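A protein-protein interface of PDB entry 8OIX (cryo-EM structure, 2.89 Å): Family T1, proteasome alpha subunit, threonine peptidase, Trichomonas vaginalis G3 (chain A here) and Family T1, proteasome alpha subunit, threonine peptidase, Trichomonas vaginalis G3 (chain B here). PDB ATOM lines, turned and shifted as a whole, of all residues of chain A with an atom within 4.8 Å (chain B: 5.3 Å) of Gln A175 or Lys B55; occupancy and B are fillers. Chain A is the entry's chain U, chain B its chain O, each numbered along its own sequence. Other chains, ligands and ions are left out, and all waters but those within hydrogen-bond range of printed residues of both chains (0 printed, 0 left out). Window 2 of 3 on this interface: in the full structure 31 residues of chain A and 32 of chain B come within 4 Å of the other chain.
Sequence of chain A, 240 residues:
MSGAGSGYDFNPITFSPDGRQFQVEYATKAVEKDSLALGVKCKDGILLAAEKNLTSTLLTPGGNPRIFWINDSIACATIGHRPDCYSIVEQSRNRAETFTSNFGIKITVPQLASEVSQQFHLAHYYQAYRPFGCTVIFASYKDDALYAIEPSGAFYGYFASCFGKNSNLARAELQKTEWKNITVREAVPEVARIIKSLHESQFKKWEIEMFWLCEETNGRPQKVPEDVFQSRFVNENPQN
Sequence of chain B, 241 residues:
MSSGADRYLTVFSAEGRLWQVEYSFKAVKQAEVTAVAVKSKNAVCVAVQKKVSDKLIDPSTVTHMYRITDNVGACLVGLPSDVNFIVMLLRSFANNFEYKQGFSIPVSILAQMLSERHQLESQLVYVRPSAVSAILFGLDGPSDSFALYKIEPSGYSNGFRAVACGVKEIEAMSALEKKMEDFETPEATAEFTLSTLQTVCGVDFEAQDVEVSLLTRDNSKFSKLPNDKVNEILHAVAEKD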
ATOM      1  N   PHE A 159      19.905  -1.596 -21.555  1.00  0.00           N
ATOM      2  CA  PHE A 159      20.799  -1.705 -22.698  1.00  0.00           C
ATOM      3  C   PHE A 159      21.675  -0.465 -22.801  1.00  0.00           C
ATOM      4  O   PHE A 159      22.850  -0.553 -23.173  1.00  0.00           O
ATOM      5  CB  PHE A 159      19.997  -1.906 -23.983  1.00  0.00           C
ATOM      6  CG  PHE A 159      19.078  -3.091 -23.944  1.00  0.00           C
ATOM      7  CD1 PHE A 159      19.533  -4.323 -23.507  1.00  0.00           C
ATOM      8  CD2 PHE A 159      17.758  -2.971 -24.341  1.00  0.00           C
ATOM      9  CE1 PHE A 159      18.689  -5.413 -23.470  1.00  0.00           C
ATOM     10  CE2 PHE A 159      16.910  -4.058 -24.308  1.00  0.00           C
ATOM     11  CZ  PHE A 159      17.376  -5.280 -23.871  1.00  0.00           C
ATOM     12  N   ARG A 171      19.542   9.845 -23.148  1.00  0.00           N
ATOM     13  CA  ARG A 171      18.917   8.557 -23.423  1.00  0.00           C
ATOM     14  C   ARG A 171      18.341   8.517 -24.833  1.00  0.00           C
ATOM     15  O   ARG A 171      18.449   7.498 -25.524  1.00  0.00           O
ATOM     16  CB  ARG A 171      17.836   8.265 -22.384  1.00  0.00           C
ATOM     17  CG  ARG A 171      18.381   7.817 -21.040  1.00  0.00           C
ATOM     18  CD  ARG A 171      17.296   7.194 -20.181  1.00  0.00           C
ATOM     19  NE  ARG A 171      16.169   8.097 -19.985  1.00  0.00           N
ATOM     20  CZ  ARG A 171      15.996   8.855 -18.912  1.00  0.00           C
ATOM     21  NH1 ARG A 171      16.860   8.843 -17.910  1.00  0.00           N
ATOM     22  NH2 ARG A 171      14.929   9.646 -18.842  1.00  0.00           N
ATOM     23  N   ALA A 172      17.722   9.615 -25.274  1.00  0.00           N
ATOM     24  CA  ALA A 172      17.199   9.671 -26.636  1.00  0.00           C
ATOM     25  C   ALA A 172      18.308   9.476 -27.661  1.00  0.00           C
ATOM     26  O   ALA A 172      18.101   8.837 -28.700  1.00  0.00           O
ATOM     27  CB  ALA A 172      16.480  11.000 -26.866  1.00  0.00           C
ATOM     28  N   GLU A 173      19.493  10.025 -27.391  1.00  0.00           N
ATOM     29  CA  GLU A 173      20.615   9.860 -28.309  1.00  0.00           C
ATOM     30  C   GLU A 173      21.217   8.460 -28.223  1.00  0.00           C
ATOM     31  O   GLU A 173      21.587   7.881 -29.250  1.00  0.00           O
ATOM     32  CB  GLU A 173      21.680  10.920 -28.029  1.00  0.00           C
ATOM     33  CG  GLU A 173      22.610  11.185 -29.200  1.00  0.00           C
ATOM     34  CD  GLU A 173      21.883  11.723 -30.416  1.00  0.00           C
ATOM     35  OE1 GLU A 173      20.886  12.456 -30.241  1.00  0.00           O
ATOM     36  OE2 GLU A 173      22.306  11.411 -31.549  1.00  0.00           O
ATOM     37  N   LEU A 174      21.335   7.909 -27.011  1.00  0.00           N
ATOM     38  CA  LEU A 174      21.774   6.526 -26.854  1.00  0.00           C
ATOM     39  C   LEU A 174      20.843   5.568 -27.584  1.00  0.00           C
ATOM     40  O   LEU A 174      21.277   4.512 -28.057  1.00  0.00           O
ATOM     41  CB  LEU A 174      21.841   6.155 -25.371  1.00  0.00           C
ATOM     42  CG  LEU A 174      22.843   6.867 -24.459  1.00  0.00           C
ATOM     43  CD1 LEU A 174      22.583   6.502 -23.006  1.00  0.00           C
ATOM     44  CD2 LEU A 174      24.279   6.566 -24.840  1.00  0.00           C
ATOM     45  N   GLN A 175      19.560   5.923 -27.672  1.00  0.00           N
ATOM     46  CA  GLN A 175      18.579   5.108 -28.373  1.00  0.00           C
ATOM     47  C   GLN A 175      18.891   4.981 -29.858  1.00  0.00           C
ATOM     48  O   GLN A 175      18.477   4.000 -30.486  1.00  0.00           O
ATOM     49  CB  GLN A 175      17.192   5.719 -28.174  1.00  0.00           C
ATOM     50  CG  GLN A 175      16.023   4.800 -28.450  1.00  0.00           C
ATOM     51  CD  GLN A 175      14.695   5.475 -28.161  1.00  0.00           C
ATOM     52  OE1 GLN A 175      13.771   5.427 -28.972  1.00  0.00           O
ATOM     53  NE2 GLN A 175      14.597   6.114 -27.002  1.00  0.00           N
ATOM     54  N   LYS A 176      19.611   5.947 -30.432  1.00  0.00           N
ATOM     55  CA  LYS A 176      19.873   5.957 -31.866  1.00  0.00           C
ATOM     56  C   LYS A 176      20.893   4.910 -32.295  1.00  0.00           C
ATOM     57  O   LYS A 176      21.062   4.697 -33.499  1.00  0.00           O
ATOM     58  CB  LYS A 176      20.358   7.341 -32.300  1.00  0.00           C
ATOM     59  CG  LYS A 176      19.430   8.479 -31.915  1.00  0.00           C
ATOM     60  CD  LYS A 176      18.008   8.229 -32.384  1.00  0.00           C
ATOM     61  CE  LYS A 176      17.198   9.517 -32.385  1.00  0.00           C
ATOM     62  NZ  LYS A 176      17.338  10.265 -31.105  1.00  0.00           N
ATOM     63  N   THR A 177      21.570   4.259 -31.354  1.00  0.00           N
ATOM     64  CA  THR A 177      22.635   3.316 -31.664  1.00  0.00           C
ATOM     65  C   THR A 177      22.317   1.953 -31.067  1.00  0.00           C
ATOM     66  O   THR A 177      21.897   1.854 -29.909  1.00  0.00           O
ATOM     67  CB  THR A 177      23.985   3.821 -31.132  1.00  0.00           C
ATOM     68  OG1 THR A 177      24.411   4.952 -31.900  1.00  0.00           O
ATOM     69  CG2 THR A 177      25.045   2.735 -31.216  1.00  0.00           C
ATOM     70  N   TRP A 179      24.001  -0.557 -29.500  1.00  0.00           N
ATOM     71  CA  TRP A 179      25.327  -0.571 -28.891  1.00  0.00           C
ATOM     72  C   TRP A 179      25.931  -1.970 -28.875  1.00  0.00           C
ATOM     73  O   TRP A 179      27.150  -2.122 -29.012  1.00  0.00           O
ATOM     74  CB  TRP A 179      25.252   0.012 -27.482  1.00  0.00           C
ATOM     75  CG  TRP A 179      24.779   1.429 -27.476  1.00  0.00           C
ATOM     76  CD1 TRP A 179      23.505   1.867 -27.270  1.00  0.00           C
ATOM     77  CD2 TRP A 179      25.571   2.596 -27.719  1.00  0.00           C
ATOM     78  NE1 TRP A 179      23.455   3.236 -27.355  1.00  0.00           N
ATOM     79  CE2 TRP A 179      24.712   3.707 -27.631  1.00  0.00           C
ATOM     80  CE3 TRP A 179      26.924   2.809 -27.996  1.00  0.00           C
ATOM     81  CZ2 TRP A 179      25.161   5.013 -27.812  1.00  0.00           C
ATOM     82  CZ3 TRP A 179      27.368   4.105 -28.173  1.00  0.00           C
ATOM     83  CH2 TRP A 179      26.489   5.190 -28.080  1.00  0.00           C
ATOM     84  N   VAL B  52       6.938  -1.035 -20.133  1.00  0.00           N
ATOM     85  CA  VAL B  52       8.300  -0.515 -20.157  1.00  0.00           C
ATOM     86  C   VAL B  52       8.241   0.883 -20.765  1.00  0.00           C
ATOM     87  O   VAL B  52       7.992   1.036 -21.963  1.00  0.00           O
ATOM     88  CB  VAL B  52       9.238  -1.433 -20.945  1.00  0.00           C
ATOM     89  CG1 VAL B  52      10.622  -0.825 -21.036  1.00  0.00           C
ATOM     90  CG2 VAL B  52       9.300  -2.807 -20.295  1.00  0.00           C
ATOM     91  N   SER B  53       8.462   1.905 -19.934  1.00  0.00           N
ATOM     92  CA  SER B  53       8.316   3.284 -20.395  1.00  0.00           C
ATOM     93  C   SER B  53       9.324   3.619 -21.489  1.00  0.00           C
ATOM     94  O   SER B  53       8.964   4.195 -22.523  1.00  0.00           O
ATOM     95  CB  SER B  53       8.464   4.246 -19.215  1.00  0.00           C
ATOM     96  OG  SER B  53       8.242   5.586 -19.620  1.00  0.00           O
ATOM     97  N   ASP B  54      10.589   3.265 -21.283  1.00  0.00           N
ATOM     98  CA  ASP B  54      11.647   3.535 -22.247  1.00  0.00           C
ATOM     99  C   ASP B  54      12.264   2.220 -22.694  1.00  0.00           C
ATOM    100  O   ASP B  54      12.674   1.409 -21.858  1.00  0.00           O
ATOM    101  CB  ASP B  54      12.719   4.450 -21.651  1.00  0.00           C
ATOM    102  CG  ASP B  54      12.332   5.915 -21.711  1.00  0.00           C
ATOM    103  OD1 ASP B  54      11.454   6.263 -22.529  1.00  0.00           O
ATOM    104  OD2 ASP B  54      12.904   6.716 -20.943  1.00  0.00           O
ATOM    105  N   LYS B  55      12.355   2.021 -24.010  1.00  0.00           N
ATOM    106  CA  LYS B  55      12.890   0.766 -24.525  1.00  0.00           C
ATOM    107  C   LYS B  55      14.403   0.657 -24.385  1.00  0.00           C
ATOM    108  O   LYS B  55      14.965  -0.368 -24.785  1.00  0.00           O
ATOM    109  CB  LYS B  55      12.482   0.570 -25.987  1.00  0.00           C
ATOM    110  CG  LYS B  55      12.915   1.669 -26.936  1.00  0.00           C
ATOM    111  CD  LYS B  55      12.488   1.329 -28.356  1.00  0.00           C
ATOM    112  CE  LYS B  55      12.767   2.467 -29.316  1.00  0.00           C
ATOM    113  NZ  LYS B  55      12.396   2.113 -30.714  1.00  0.00           N
ATOM    114  N   LEU B  56      15.077   1.673 -23.842  1.00  0.00           N
ATOM    115  CA  LEU B  56      16.476   1.503 -23.470  1.00  0.00           C
ATOM    116  C   LEU B  56      16.631   0.550 -22.296  1.00  0.00           C
ATOM    117  O   LEU B  56      17.695  -0.056 -22.136  1.00  0.00           O
ATOM    118  CB  LEU B  56      17.110   2.852 -23.125  1.00  0.00           C
ATOM    119  CG  LEU B  56      17.240   3.881 -24.247  1.00  0.00           C
ATOM    120  CD1 LEU B  56      16.068   4.848 -24.237  1.00  0.00           C
ATOM    121  CD2 LEU B  56      18.557   4.626 -24.129  1.00  0.00           C
ATOM    122  N   ILE B  57      15.591   0.412 -21.473  1.00  0.00           N
ATOM    123  CA  ILE B  57      15.637  -0.488 -20.331  1.00  0.00           C
ATOM    124  C   ILE B  57      15.553  -1.927 -20.816  1.00  0.00           C
ATOM    125  O   ILE B  57      14.758  -2.256 -21.707  1.00  0.00           O
ATOM    126  CB  ILE B  57      14.492  -0.169 -19.355  1.00  0.00           C
ATOM    127  CG1 ILE B  57      14.448   1.327 -19.049  1.00  0.00           C
ATOM    128  CG2 ILE B  57      14.670  -0.937 -18.068  1.00  0.00           C
ATOM    129  CD1 ILE B  57      13.247   1.743 -18.232  1.00  0.00           C
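OD2 of Asp B54 lies within salt-bridge range of NE of Arg A171 (3.7 Å).
O of Leu B56 is in hydrogen-bond range of N of Phe A159, at 2.8 Å.
The indole nitrogen of Trp A179 sits at hydrogen-bond distance from the backbone carbonyl oxygen of Leu A174 (2.6 Å).
Lys B55 touches Phe A159 (O to CD2, 3.8 Å).
CE2 of Phe A159 touches O of Ile B57 (3.8 Å).
Leu B56 touches Arg A171.
Leu B56 touches Leu A174 (CD2 to CB, 3.8 Å).
Gln A175 touches Lys B55 (OE1 to CE, 3.1 Å).
Gln A175 touches Leu B56 (NE2 to CD1, 3.4 Å).
Gln A175 touches just these residues of chain B: Lys B55 and Leu B56.
Of the printed residues of chain A, Lys B55 touches Phe A159 (3.8 Å) and Gln A175 (3.1 Å).
Printed residues of chain A within 4 Å of Leu B56: Phe A159 (2.8 Å), Arg A171 (3.2 Å), Leu A174 (3.8 Å) and Gln A175 (3.4 Å).
Printed residues of chain A within 4 Å of Asp B54: Arg A171.
Glu A173 touches none of the printed residues of chain B.
The nearest printed residue of chain B that does not touch Gln A175 is Asp B54 (5.5 Å).
The nearest printed residue of chain A that does not touch Lys B55 is Lys A176 (7.8 Å).
Of the 9 printed residues of chain A, 4 touch a printed residue of chain B.
Hydrophobic or aromatic side chains of chain A within 4 Å of the printed part of chain B: Phe A159 and Leu A174.
Hydrophobic or aromatic side chains of chain B that line the printed part of chain A: Leu B56.
Among the printed residues, 8 pairs touch across the chains.
Among the printed residues, Asp or Glu carboxylates within 4 Å of a Lys or Arg side-chain nitrogen of the other chain: Arg A171 with Asp B54 (3.7 Å).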
